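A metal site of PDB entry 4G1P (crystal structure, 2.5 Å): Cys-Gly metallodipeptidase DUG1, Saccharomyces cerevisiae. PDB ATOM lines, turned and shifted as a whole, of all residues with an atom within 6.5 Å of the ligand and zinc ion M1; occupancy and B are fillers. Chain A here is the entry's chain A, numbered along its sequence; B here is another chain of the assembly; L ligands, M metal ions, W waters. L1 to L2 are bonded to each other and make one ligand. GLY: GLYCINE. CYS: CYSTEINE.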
ATOM      1  N   HIS A 102      -9.920 -11.579   3.795  1.00  0.00           N
ATOM      2  CA  HIS A 102     -10.141 -11.460   5.229  1.00  0.00           C
ATOM      3  C   HIS A 102      -9.380 -12.471   6.028  1.00  0.00           C
ATOM      4  O   HIS A 102      -9.286 -13.653   5.650  1.00  0.00           O
ATOM      5  CB  HIS A 102     -11.637 -11.478   5.573  1.00  0.00           C
ATOM      6  CG  HIS A 102     -12.311 -12.798   5.345  1.00  0.00           C
ATOM      7  ND1 HIS A 102     -12.364 -13.775   6.314  1.00  0.00           N
ATOM      8  CD2 HIS A 102     -13.017 -13.277   4.294  1.00  0.00           C
ATOM      9  CE1 HIS A 102     -13.046 -14.807   5.851  1.00  0.00           C
ATOM     10  NE2 HIS A 102     -13.457 -14.532   4.629  1.00  0.00           N
ATOM     11  N   GLN A 106     -14.111 -18.530  10.969  1.00  0.00           N
ATOM     12  CA  GLN A 106     -15.182 -19.166  11.750  1.00  0.00           C
ATOM     13  C   GLN A 106     -14.628 -19.920  12.970  1.00  0.00           C
ATOM     14  O   GLN A 106     -13.505 -20.385  12.950  1.00  0.00           O
ATOM     15  CB  GLN A 106     -15.963 -20.132  10.854  1.00  0.00           C
ATOM     16  CG  GLN A 106     -16.856 -19.448   9.841  1.00  0.00           C
ATOM     17  CD  GLN A 106     -18.087 -18.849  10.475  1.00  0.00           C
ATOM     18  OE1 GLN A 106     -18.789 -19.517  11.228  1.00  0.00           O
ATOM     19  NE2 GLN A 106     -18.354 -17.563  10.189  1.00  0.00           N
ATOM     20  N   ASP A 137     -11.149 -20.265   3.585  1.00  0.00           N
ATOM     21  CA  ASP A 137     -12.015 -19.139   3.882  1.00  0.00           C
ATOM     22  C   ASP A 137     -11.454 -18.433   5.108  1.00  0.00           C
ATOM     23  O   ASP A 137     -11.908 -18.714   6.221  1.00  0.00           O
ATOM     24  CB  ASP A 137     -13.440 -19.663   4.145  1.00  0.00           C
ATOM     25  CG  ASP A 137     -14.429 -18.562   4.490  1.00  0.00           C
ATOM     26  OD1 ASP A 137     -14.117 -17.370   4.305  1.00  0.00           O
ATOM     27  OD2 ASP A 137     -15.554 -18.887   4.927  1.00  0.00           O
ATOM     28  N   ASP A 138     -10.504 -17.519   4.925  1.00  0.00           N
ATOM     29  CA  ASP A 138     -10.064 -16.992   3.641  1.00  0.00           C
ATOM     30  C   ASP A 138      -8.546 -16.817   3.647  1.00  0.00           C
ATOM     31  O   ASP A 138      -7.998 -16.061   2.860  1.00  0.00           O
ATOM     32  CB  ASP A 138     -10.737 -15.623   3.403  1.00  0.00           C
ATOM     33  CG  ASP A 138     -10.476 -15.032   2.008  1.00  0.00           C
ATOM     34  OD1 ASP A 138     -10.530 -15.766   0.995  1.00  0.00           O
ATOM     35  OD2 ASP A 138     -10.215 -13.810   1.922  1.00  0.00           O
ATOM     36  N   GLU A 171     -14.847 -10.196   8.691  1.00  0.00           N
ATOM     37  CA  GLU A 171     -15.711 -10.691   7.627  1.00  0.00           C
ATOM     38  C   GLU A 171     -16.709 -11.725   8.132  1.00  0.00           C
ATOM     39  O   GLU A 171     -17.859 -11.746   7.705  1.00  0.00           O
ATOM     40  CB  GLU A 171     -14.917 -11.255   6.457  1.00  0.00           C
ATOM     41  CG  GLU A 171     -15.651 -11.273   5.123  1.00  0.00           C
ATOM     42  CD  GLU A 171     -16.351 -12.595   4.824  1.00  0.00           C
ATOM     43  OE1 GLU A 171     -16.365 -13.497   5.686  1.00  0.00           O
ATOM     44  OE2 GLU A 171     -16.908 -12.728   3.702  1.00  0.00           O
ATOM     45  N   GLU A 172     -16.276 -12.563   9.069  1.00  0.00           N
ATOM     46  CA  GLU A 172     -17.147 -13.603   9.609  1.00  0.00           C
ATOM     47  C   GLU A 172     -18.066 -13.033  10.698  1.00  0.00           C
ATOM     48  O   GLU A 172     -18.818 -13.777  11.333  1.00  0.00           O
ATOM     49  CB  GLU A 172     -16.321 -14.778  10.144  1.00  0.00           C
ATOM     50  CG  GLU A 172     -15.341 -15.396   9.151  1.00  0.00           C
ATOM     51  CD  GLU A 172     -16.028 -16.241   8.085  1.00  0.00           C
ATOM     52  OE1 GLU A 172     -17.269 -16.363   8.115  1.00  0.00           O
ATOM     53  OE2 GLU A 172     -15.320 -16.792   7.213  1.00  0.00           O
ATOM     54  N   SER A 173     -18.000 -11.726  10.893  1.00  0.00           N
ATOM     55  CA  SER A 173     -18.766 -11.051  11.939  1.00  0.00           C
ATOM     56  C   SER A 173     -19.382  -9.740  11.422  1.00  0.00           C
ATOM     57  O   SER A 173     -19.348  -8.711  12.102  1.00  0.00           O
ATOM     58  CB  SER A 173     -17.872 -10.784  13.152  1.00  0.00           C
ATOM     59  OG  SER A 173     -17.255 -11.973  13.616  1.00  0.00           O
ATOM     60  N   GLY A 174     -19.909  -9.788  10.202  1.00  0.00           N
ATOM     61  CA  GLY A 174     -20.615  -8.652   9.632  1.00  0.00           C
ATOM     62  C   GLY A 174     -19.797  -7.590   8.923  1.00  0.00           C
ATOM     63  O   GLY A 174     -20.367  -6.603   8.452  1.00  0.00           O
ATOM     64  N   ASP A 200     -12.404 -14.990  -2.628  1.00  0.00           N
ATOM     65  CA  ASP A 200     -13.099 -15.293  -1.385  1.00  0.00           C
ATOM     66  C   ASP A 200     -14.333 -16.137  -1.641  1.00  0.00           C
ATOM     67  O   ASP A 200     -15.357 -15.981  -0.966  1.00  0.00           O
ATOM     68  CB  ASP A 200     -13.506 -13.991  -0.705  1.00  0.00           C
ATOM     69  CG  ASP A 200     -13.575 -14.112   0.808  1.00  0.00           C
ATOM     70  OD1 ASP A 200     -13.362 -15.220   1.344  1.00  0.00           O
ATOM     71  OD2 ASP A 200     -13.850 -13.099   1.471  1.00  0.00           O
ATOM     72  N   TYR A 202     -15.479 -20.028  -4.179  1.00  0.00           N
ATOM     73  CA  TYR A 202     -15.046 -21.368  -4.592  1.00  0.00           C
ATOM     74  C   TYR A 202     -15.580 -21.693  -5.962  1.00  0.00           C
ATOM     75  O   TYR A 202     -16.535 -21.063  -6.421  1.00  0.00           O
ATOM     76  CB  TYR A 202     -15.556 -22.418  -3.602  1.00  0.00           C
ATOM     77  CG  TYR A 202     -15.639 -21.830  -2.218  1.00  0.00           C
ATOM     78  CD1 TYR A 202     -16.793 -21.183  -1.785  1.00  0.00           C
ATOM     79  CD2 TYR A 202     -14.534 -21.848  -1.374  1.00  0.00           C
ATOM     80  CE1 TYR A 202     -16.851 -20.585  -0.535  1.00  0.00           C
ATOM     81  CE2 TYR A 202     -14.590 -21.270  -0.130  1.00  0.00           C
ATOM     82  CZ  TYR A 202     -15.743 -20.645   0.296  1.00  0.00           C
ATOM     83  OH  TYR A 202     -15.792 -20.051   1.549  1.00  0.00           O
ATOM     84  N   CYS A 218     -27.048 -11.115   2.172  1.00  0.00           N
ATOM     85  CA  CYS A 218     -27.427 -11.874   3.353  1.00  0.00           C
ATOM     86  C   CYS A 218     -27.985 -10.960   4.449  1.00  0.00           C
ATOM     87  O   CYS A 218     -27.351  -9.979   4.862  1.00  0.00           O
ATOM     88  CB  CYS A 218     -26.244 -12.703   3.871  1.00  0.00           C
ATOM     89  SG  CYS A 218     -26.683 -13.845   5.225  1.00  0.00           S
ATOM     90  N   ASN A 219     -29.190 -11.272   4.898  1.00  0.00           N
ATOM     91  CA  ASN A 219     -29.786 -10.561   6.027  1.00  0.00           C
ATOM     92  C   ASN A 219     -29.933 -11.532   7.196  1.00  0.00           C
ATOM     93  O   ASN A 219     -30.616 -12.561   7.079  1.00  0.00           O
ATOM     94  CB  ASN A 219     -31.132  -9.938   5.642  1.00  0.00           C
ATOM     95  CG  ASN A 219     -30.969  -8.648   4.860  1.00  0.00           C
ATOM     96  OD1 ASN A 219     -29.961  -8.434   4.191  1.00  0.00           O
ATOM     97  ND2 ASN A 219     -31.965  -7.779   4.943  1.00  0.00           N
ATOM     98  N   TYR A 220     -29.270 -11.237   8.294  1.00  0.00           N
ATOM     99  CA  TYR A 220     -29.274 -12.173   9.404  1.00  0.00           C
ATOM    100  C   TYR A 220     -30.146 -11.644  10.537  1.00  0.00           C
ATOM    101  O   TYR A 220     -29.916 -10.530  11.039  1.00  0.00           O
ATOM    102  CB  TYR A 220     -27.849 -12.432   9.898  1.00  0.00           C
ATOM    103  CG  TYR A 220     -27.677 -13.756  10.611  1.00  0.00           C
ATOM    104  CD1 TYR A 220     -28.154 -13.937  11.895  1.00  0.00           C
ATOM    105  CD2 TYR A 220     -27.042 -14.820   9.991  1.00  0.00           C
ATOM    106  CE1 TYR A 220     -28.011 -15.149  12.549  1.00  0.00           C
ATOM    107  CE2 TYR A 220     -26.879 -16.023  10.635  1.00  0.00           C
ATOM    108  CZ  TYR A 220     -27.369 -16.186  11.917  1.00  0.00           C
ATOM    109  OH  TYR A 220     -27.208 -17.378  12.587  1.00  0.00           O
ATOM    110  N   ARG A 348     -30.921 -15.183   2.162  1.00  0.00           N
ATOM    111  CA  ARG A 348     -30.022 -14.848   1.075  1.00  0.00           C
ATOM    112  C   ARG A 348     -30.758 -13.978   0.070  1.00  0.00           C
ATOM    113  O   ARG A 348     -31.746 -14.399  -0.509  1.00  0.00           O
ATOM    114  CB  ARG A 348     -29.483 -16.115   0.412  1.00  0.00           C
ATOM    115  CG  ARG A 348     -28.605 -16.970   1.329  1.00  0.00           C
ATOM    116  CD  ARG A 348     -27.261 -16.316   1.623  1.00  0.00           C
ATOM    117  NE  ARG A 348     -26.564 -17.032   2.682  1.00  0.00           N
ATOM    118  CZ  ARG A 348     -25.314 -16.775   3.082  1.00  0.00           C
ATOM    119  NH1 ARG A 348     -24.576 -15.835   2.491  1.00  0.00           N
ATOM    120  NH2 ARG A 348     -24.791 -17.499   4.077  1.00  0.00           N
ATOM    121  N   HIS A 385     -27.116  -8.464  11.069  1.00  0.00           N
ATOM    122  CA  HIS A 385     -26.303  -7.817  10.039  1.00  0.00           C
ATOM    123  C   HIS A 385     -26.903  -7.990   8.652  1.00  0.00           C
ATOM    124  O   HIS A 385     -27.662  -8.934   8.399  1.00  0.00           O
ATOM    125  CB  HIS A 385     -24.847  -8.279  10.090  1.00  0.00           C
ATOM    126  CG  HIS A 385     -24.620  -9.680   9.626  1.00  0.00           C
ATOM    127  ND1 HIS A 385     -24.032 -10.639  10.427  1.00  0.00           N
ATOM    128  CD2 HIS A 385     -24.858 -10.291   8.436  1.00  0.00           C
ATOM    129  CE1 HIS A 385     -23.942 -11.779   9.760  1.00  0.00           C
ATOM    130  NE2 HIS A 385     -24.440 -11.594   8.548  1.00  0.00           N
ATOM    131  N   GLY A 420     -23.851 -18.590  -4.397  1.00  0.00           N
ATOM    132  CA  GLY A 420     -24.857 -18.665  -3.348  1.00  0.00           C
ATOM    133  C   GLY A 420     -24.394 -17.916  -2.109  1.00  0.00           C
ATOM    134  O   GLY A 420     -25.200 -17.358  -1.363  1.00  0.00           O
ATOM    135  N   GLY A 421     -23.084 -17.895  -1.894  1.00  0.00           N
ATOM    136  CA  GLY A 421     -22.509 -17.212  -0.750  1.00  0.00           C
ATOM    137  C   GLY A 421     -22.503 -15.707  -0.926  1.00  0.00           C
ATOM    138  O   GLY A 421     -23.028 -15.206  -1.923  1.00  0.00           O
ATOM    139  N   SER A 422     -21.881 -15.010   0.015  1.00  0.00           N
ATOM    140  CA  SER A 422     -21.900 -13.556   0.053  1.00  0.00           C
ATOM    141  C   SER A 422     -20.557 -12.963   0.397  1.00  0.00           C
ATOM    142  O   SER A 422     -19.808 -13.510   1.200  1.00  0.00           O
ATOM    143  CB  SER A 422     -22.897 -13.096   1.092  1.00  0.00           C
ATOM    144  OG  SER A 422     -24.137 -13.699   0.853  1.00  0.00           O
ATOM    145  N   ILE A 423     -20.244 -11.840  -0.214  1.00  0.00           N
ATOM    146  CA  ILE A 423     -19.095 -11.065   0.198  1.00  0.00           C
ATOM    147  C   ILE A 423     -19.554  -9.627   0.295  1.00  0.00           C
ATOM    148  O   ILE A 423     -19.395  -8.860  -0.621  1.00  0.00           O
ATOM    149  CB  ILE A 423     -17.942 -11.161  -0.788  1.00  0.00           C
ATOM    150  CG1 ILE A 423     -17.606 -12.626  -1.069  1.00  0.00           C
ATOM    151  CG2 ILE A 423     -16.747 -10.421  -0.249  1.00  0.00           C
ATOM    152  CD1 ILE A 423     -16.677 -12.841  -2.259  1.00  0.00           C
ATOM    153  N   PRO A 424     -20.160  -9.282   1.429  1.00  0.00           N
ATOM    154  CA  PRO A 424     -20.793  -7.982   1.698  1.00  0.00           C
ATOM    155  C   PRO A 424     -20.182  -6.726   1.043  1.00  0.00           C
ATOM    156  O   PRO A 424     -20.976  -5.995   0.474  1.00  0.00           O
ATOM    157  CB  PRO A 424     -20.735  -7.907   3.219  1.00  0.00           C
ATOM    158  CG  PRO A 424     -20.958  -9.330   3.629  1.00  0.00           C
ATOM    159  CD  PRO A 424     -20.267 -10.182   2.593  1.00  0.00           C
ATOM    160  N   ALA A 449     -16.020 -24.935   3.881  1.00  0.00           N
ATOM    161  CA  ALA A 449     -16.045 -23.667   4.598  1.00  0.00           C
ATOM    162  C   ALA A 449     -17.234 -23.622   5.573  1.00  0.00           C
ATOM    163  O   ALA A 449     -18.330 -24.095   5.249  1.00  0.00           O
ATOM    164  CB  ALA A 449     -16.103 -22.498   3.636  1.00  0.00           C
ATOM    165  N   HIS A 450     -16.981 -23.091   6.767  1.00  0.00           N
ATOM    166  CA  HIS A 450     -17.983 -22.974   7.833  1.00  0.00           C
ATOM    167  C   HIS A 450     -18.393 -24.335   8.379  1.00  0.00           C
ATOM    168  O   HIS A 450     -19.424 -24.465   9.040  1.00  0.00           O
ATOM    169  CB  HIS A 450     -19.224 -22.205   7.360  1.00  0.00           C
ATOM    170  CG  HIS A 450     -18.945 -20.782   7.001  1.00  0.00           C
ATOM    171  ND1 HIS A 450     -19.939 -19.828   6.962  1.00  0.00           N
ATOM    172  CD2 HIS A 450     -17.801 -20.147   6.661  1.00  0.00           C
ATOM    173  CE1 HIS A 450     -19.415 -18.660   6.618  1.00  0.00           C
ATOM    174  NE2 HIS A 450     -18.117 -18.834   6.429  1.00  0.00           N
ATOM    175  N   HIS B 233     -22.345 -24.699   4.691  1.00  0.00           N
ATOM    176  CA  HIS B 233     -22.357 -23.244   4.559  1.00  0.00           C
ATOM    177  C   HIS B 233     -23.757 -22.862   4.082  1.00  0.00           C
ATOM    178  O   HIS B 233     -24.221 -23.354   3.063  1.00  0.00           O
ATOM    179  CB  HIS B 233     -21.300 -22.815   3.543  1.00  0.00           C
ATOM    180  CG  HIS B 233     -21.143 -21.330   3.411  1.00  0.00           C
ATOM    181  ND1 HIS B 233     -22.143 -20.529   2.904  1.00  0.00           N
ATOM    182  CD2 HIS B 233     -20.118 -20.510   3.731  1.00  0.00           C
ATOM    183  CE1 HIS B 233     -21.725 -19.270   2.907  1.00  0.00           C
ATOM    184  NE2 HIS B 233     -20.505 -19.230   3.408  1.00  0.00           N
ATOM    185  N   SER B 234     -24.440 -22.009   4.832  1.00  0.00           N
ATOM    186  CA  SER B 234     -25.848 -21.804   4.526  1.00  0.00           C
ATOM    187  C   SER B 234     -26.070 -20.986   3.256  1.00  0.00           C
ATOM    188  O   SER B 234     -27.201 -20.881   2.799  1.00  0.00           O
ATOM    189  CB  SER B 234     -26.622 -21.195   5.709  1.00  0.00           C
ATOM    190  OG  SER B 234     -26.387 -19.807   5.803  1.00  0.00           O
ATOM    191  N   GLY B 235     -24.977 -20.432   2.715  1.00  0.00           N
ATOM    192  CA  GLY B 235     -25.036 -19.624   1.510  1.00  0.00           C
ATOM    193  C   GLY B 235     -24.786 -20.454   0.268  1.00  0.00           C
ATOM    194  O   GLY B 235     -25.484 -20.337  -0.728  1.00  0.00           O
ATOM    195  N   THR B 335     -23.744 -18.510   9.895  1.00  0.00           N
ATOM    196  CA  THR B 335     -24.420 -18.869   8.654  1.00  0.00           C
ATOM    197  C   THR B 335     -24.114 -20.313   8.354  1.00  0.00           C
ATOM    198  O   THR B 335     -23.232 -20.617   7.540  1.00  0.00           O
ATOM    199  CB  THR B 335     -23.943 -18.027   7.489  1.00  0.00           C
ATOM    200  OG1 THR B 335     -22.536 -17.830   7.587  1.00  0.00           O
ATOM    201  CG2 THR B 335     -24.619 -16.680   7.486  1.00  0.00           C
HETATM  202  N   GLY L   1     -18.391 -17.258   3.884  1.00  0.00           N
HETATM  203  CA  GLY L   1     -17.992 -16.016   4.520  1.00  0.00           C
HETATM  204  C   GLY L   1     -19.274 -15.265   4.750  1.00  0.00           C
HETATM  205  O   GLY L   1     -19.581 -14.291   4.056  1.00  0.00           O
HETATM  206  N   CYS L   2     -20.039 -15.741   5.731  1.00  0.00           N
HETATM  207  CA  CYS L   2     -21.424 -15.347   5.901  1.00  0.00           C
HETATM  208  C   CYS L   2     -22.250 -15.899   4.734  1.00  0.00           C
HETATM  209  O   CYS L   2     -21.938 -15.668   3.571  1.00  0.00           O
HETATM  210  CB  CYS L   2     -21.545 -13.821   6.016  1.00  0.00           C
HETATM  211  SG  CYS L   2     -23.191 -13.245   6.280  1.00  0.00           S
HETATM  212 ZN    ZN M   1     -16.707 -17.500   5.839  1.00  0.00          ZN
HETATM  213 ZN    ZN M   2     -15.718 -16.335   2.169  1.00  0.00          ZN
HETATM  214  O   HOH W   1     -20.400 -12.135   8.753  1.00  0.00           O
HETATM  215  O   HOH W   2     -24.030 -10.680   4.944  1.00  0.00           O
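Within 4 Å of zinc ion M1: Asp 137, Glu 172 and His 450. The nearest printed residue that does not touch zinc ion M1 is Glu 171 (4.02 Å).
O of GLY L1 lies close to OE2 of Glu 171 (3.1 Å). The backbone carbonyl oxygen (O) of Ser 422 sits close to an oxygen (O) of GLY L1 (3.0 Å). Residues that only touch the ligand: Thr 335 of chain B. Hydrophobic or aromatic side chains that line the ligand: His 385, His 450 and His 233 of chain B. Ten residues have an atom within 4 Å of the ligand: Asp 137, Glu 171, Glu 172, Cys 218, Arg 348, His 385, Ser 422, His 450, His 233 of chain B and Thr 335 of chain B.
Water W2 lies within hydrogen-bond range of a sulfur (SG) of CYS L2 and the backbone carbonyl oxygen of Cys 218.
OG1 of Thr 335 of chain B sits at hydrogen-bond distance from ND1 of His 450 (3.3 Å). A ring nitrogen (NE2) of His 102 sits at hydrogen-bond distance from the side-chain carboxylate of Asp 137 (2.9 Å). The backbone NH (N) of Tyr 220 lies within hydrogen-bond range of the backbone carbonyl oxygen (O) of His 385 (2.8 Å). The backbone NH (N) of Ser 234 of chain B lies within hydrogen-bond range of the backbone carbonyl oxygen (O) of Thr 335 of chain B (3.3 Å). N of Gly 235 of chain B is in hydrogen-bond range of ND1 of His 233 of chain B (2.8 Å). NE2 of Gln 106 lies within hydrogen-bond range of OE1 of Glu 172, 2.6 Å away. A ring nitrogen (NE2) of His 102 lies within hydrogen-bond range of the side-chain carboxylate (OE1) of Glu 171, at 3.3 Å. The guanidinium group (NH2) of Arg 348 lies within hydrogen-bond range of the side-chain hydroxyl (OG) of Ser 234 of chain B.
Zinc ion M1 is bound by OD2 of Asp 137 (2.0 Å), NE2 of His 450 (2.0 Å), OE2 of Glu 172 (2.1 Å) and N of GLY L1 (2.6 Å). Slightly farther from zinc ion M1 lies OE1 of Glu 172 (2.6 Å).
O of CYS L2 is in hydrogen-bond range of NH1 of Arg 348. SG of CYS L2 sits close to NE2 of His 385, 3.1 Å away. The side-chain sulfur (SG) of Cys 218 sits close to a sulfur (SG) of CYS L2. A nitrogen (N) of GLY L1 lies close to a ring nitrogen (NE2) of His 233 of chain B (2.9 Å).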
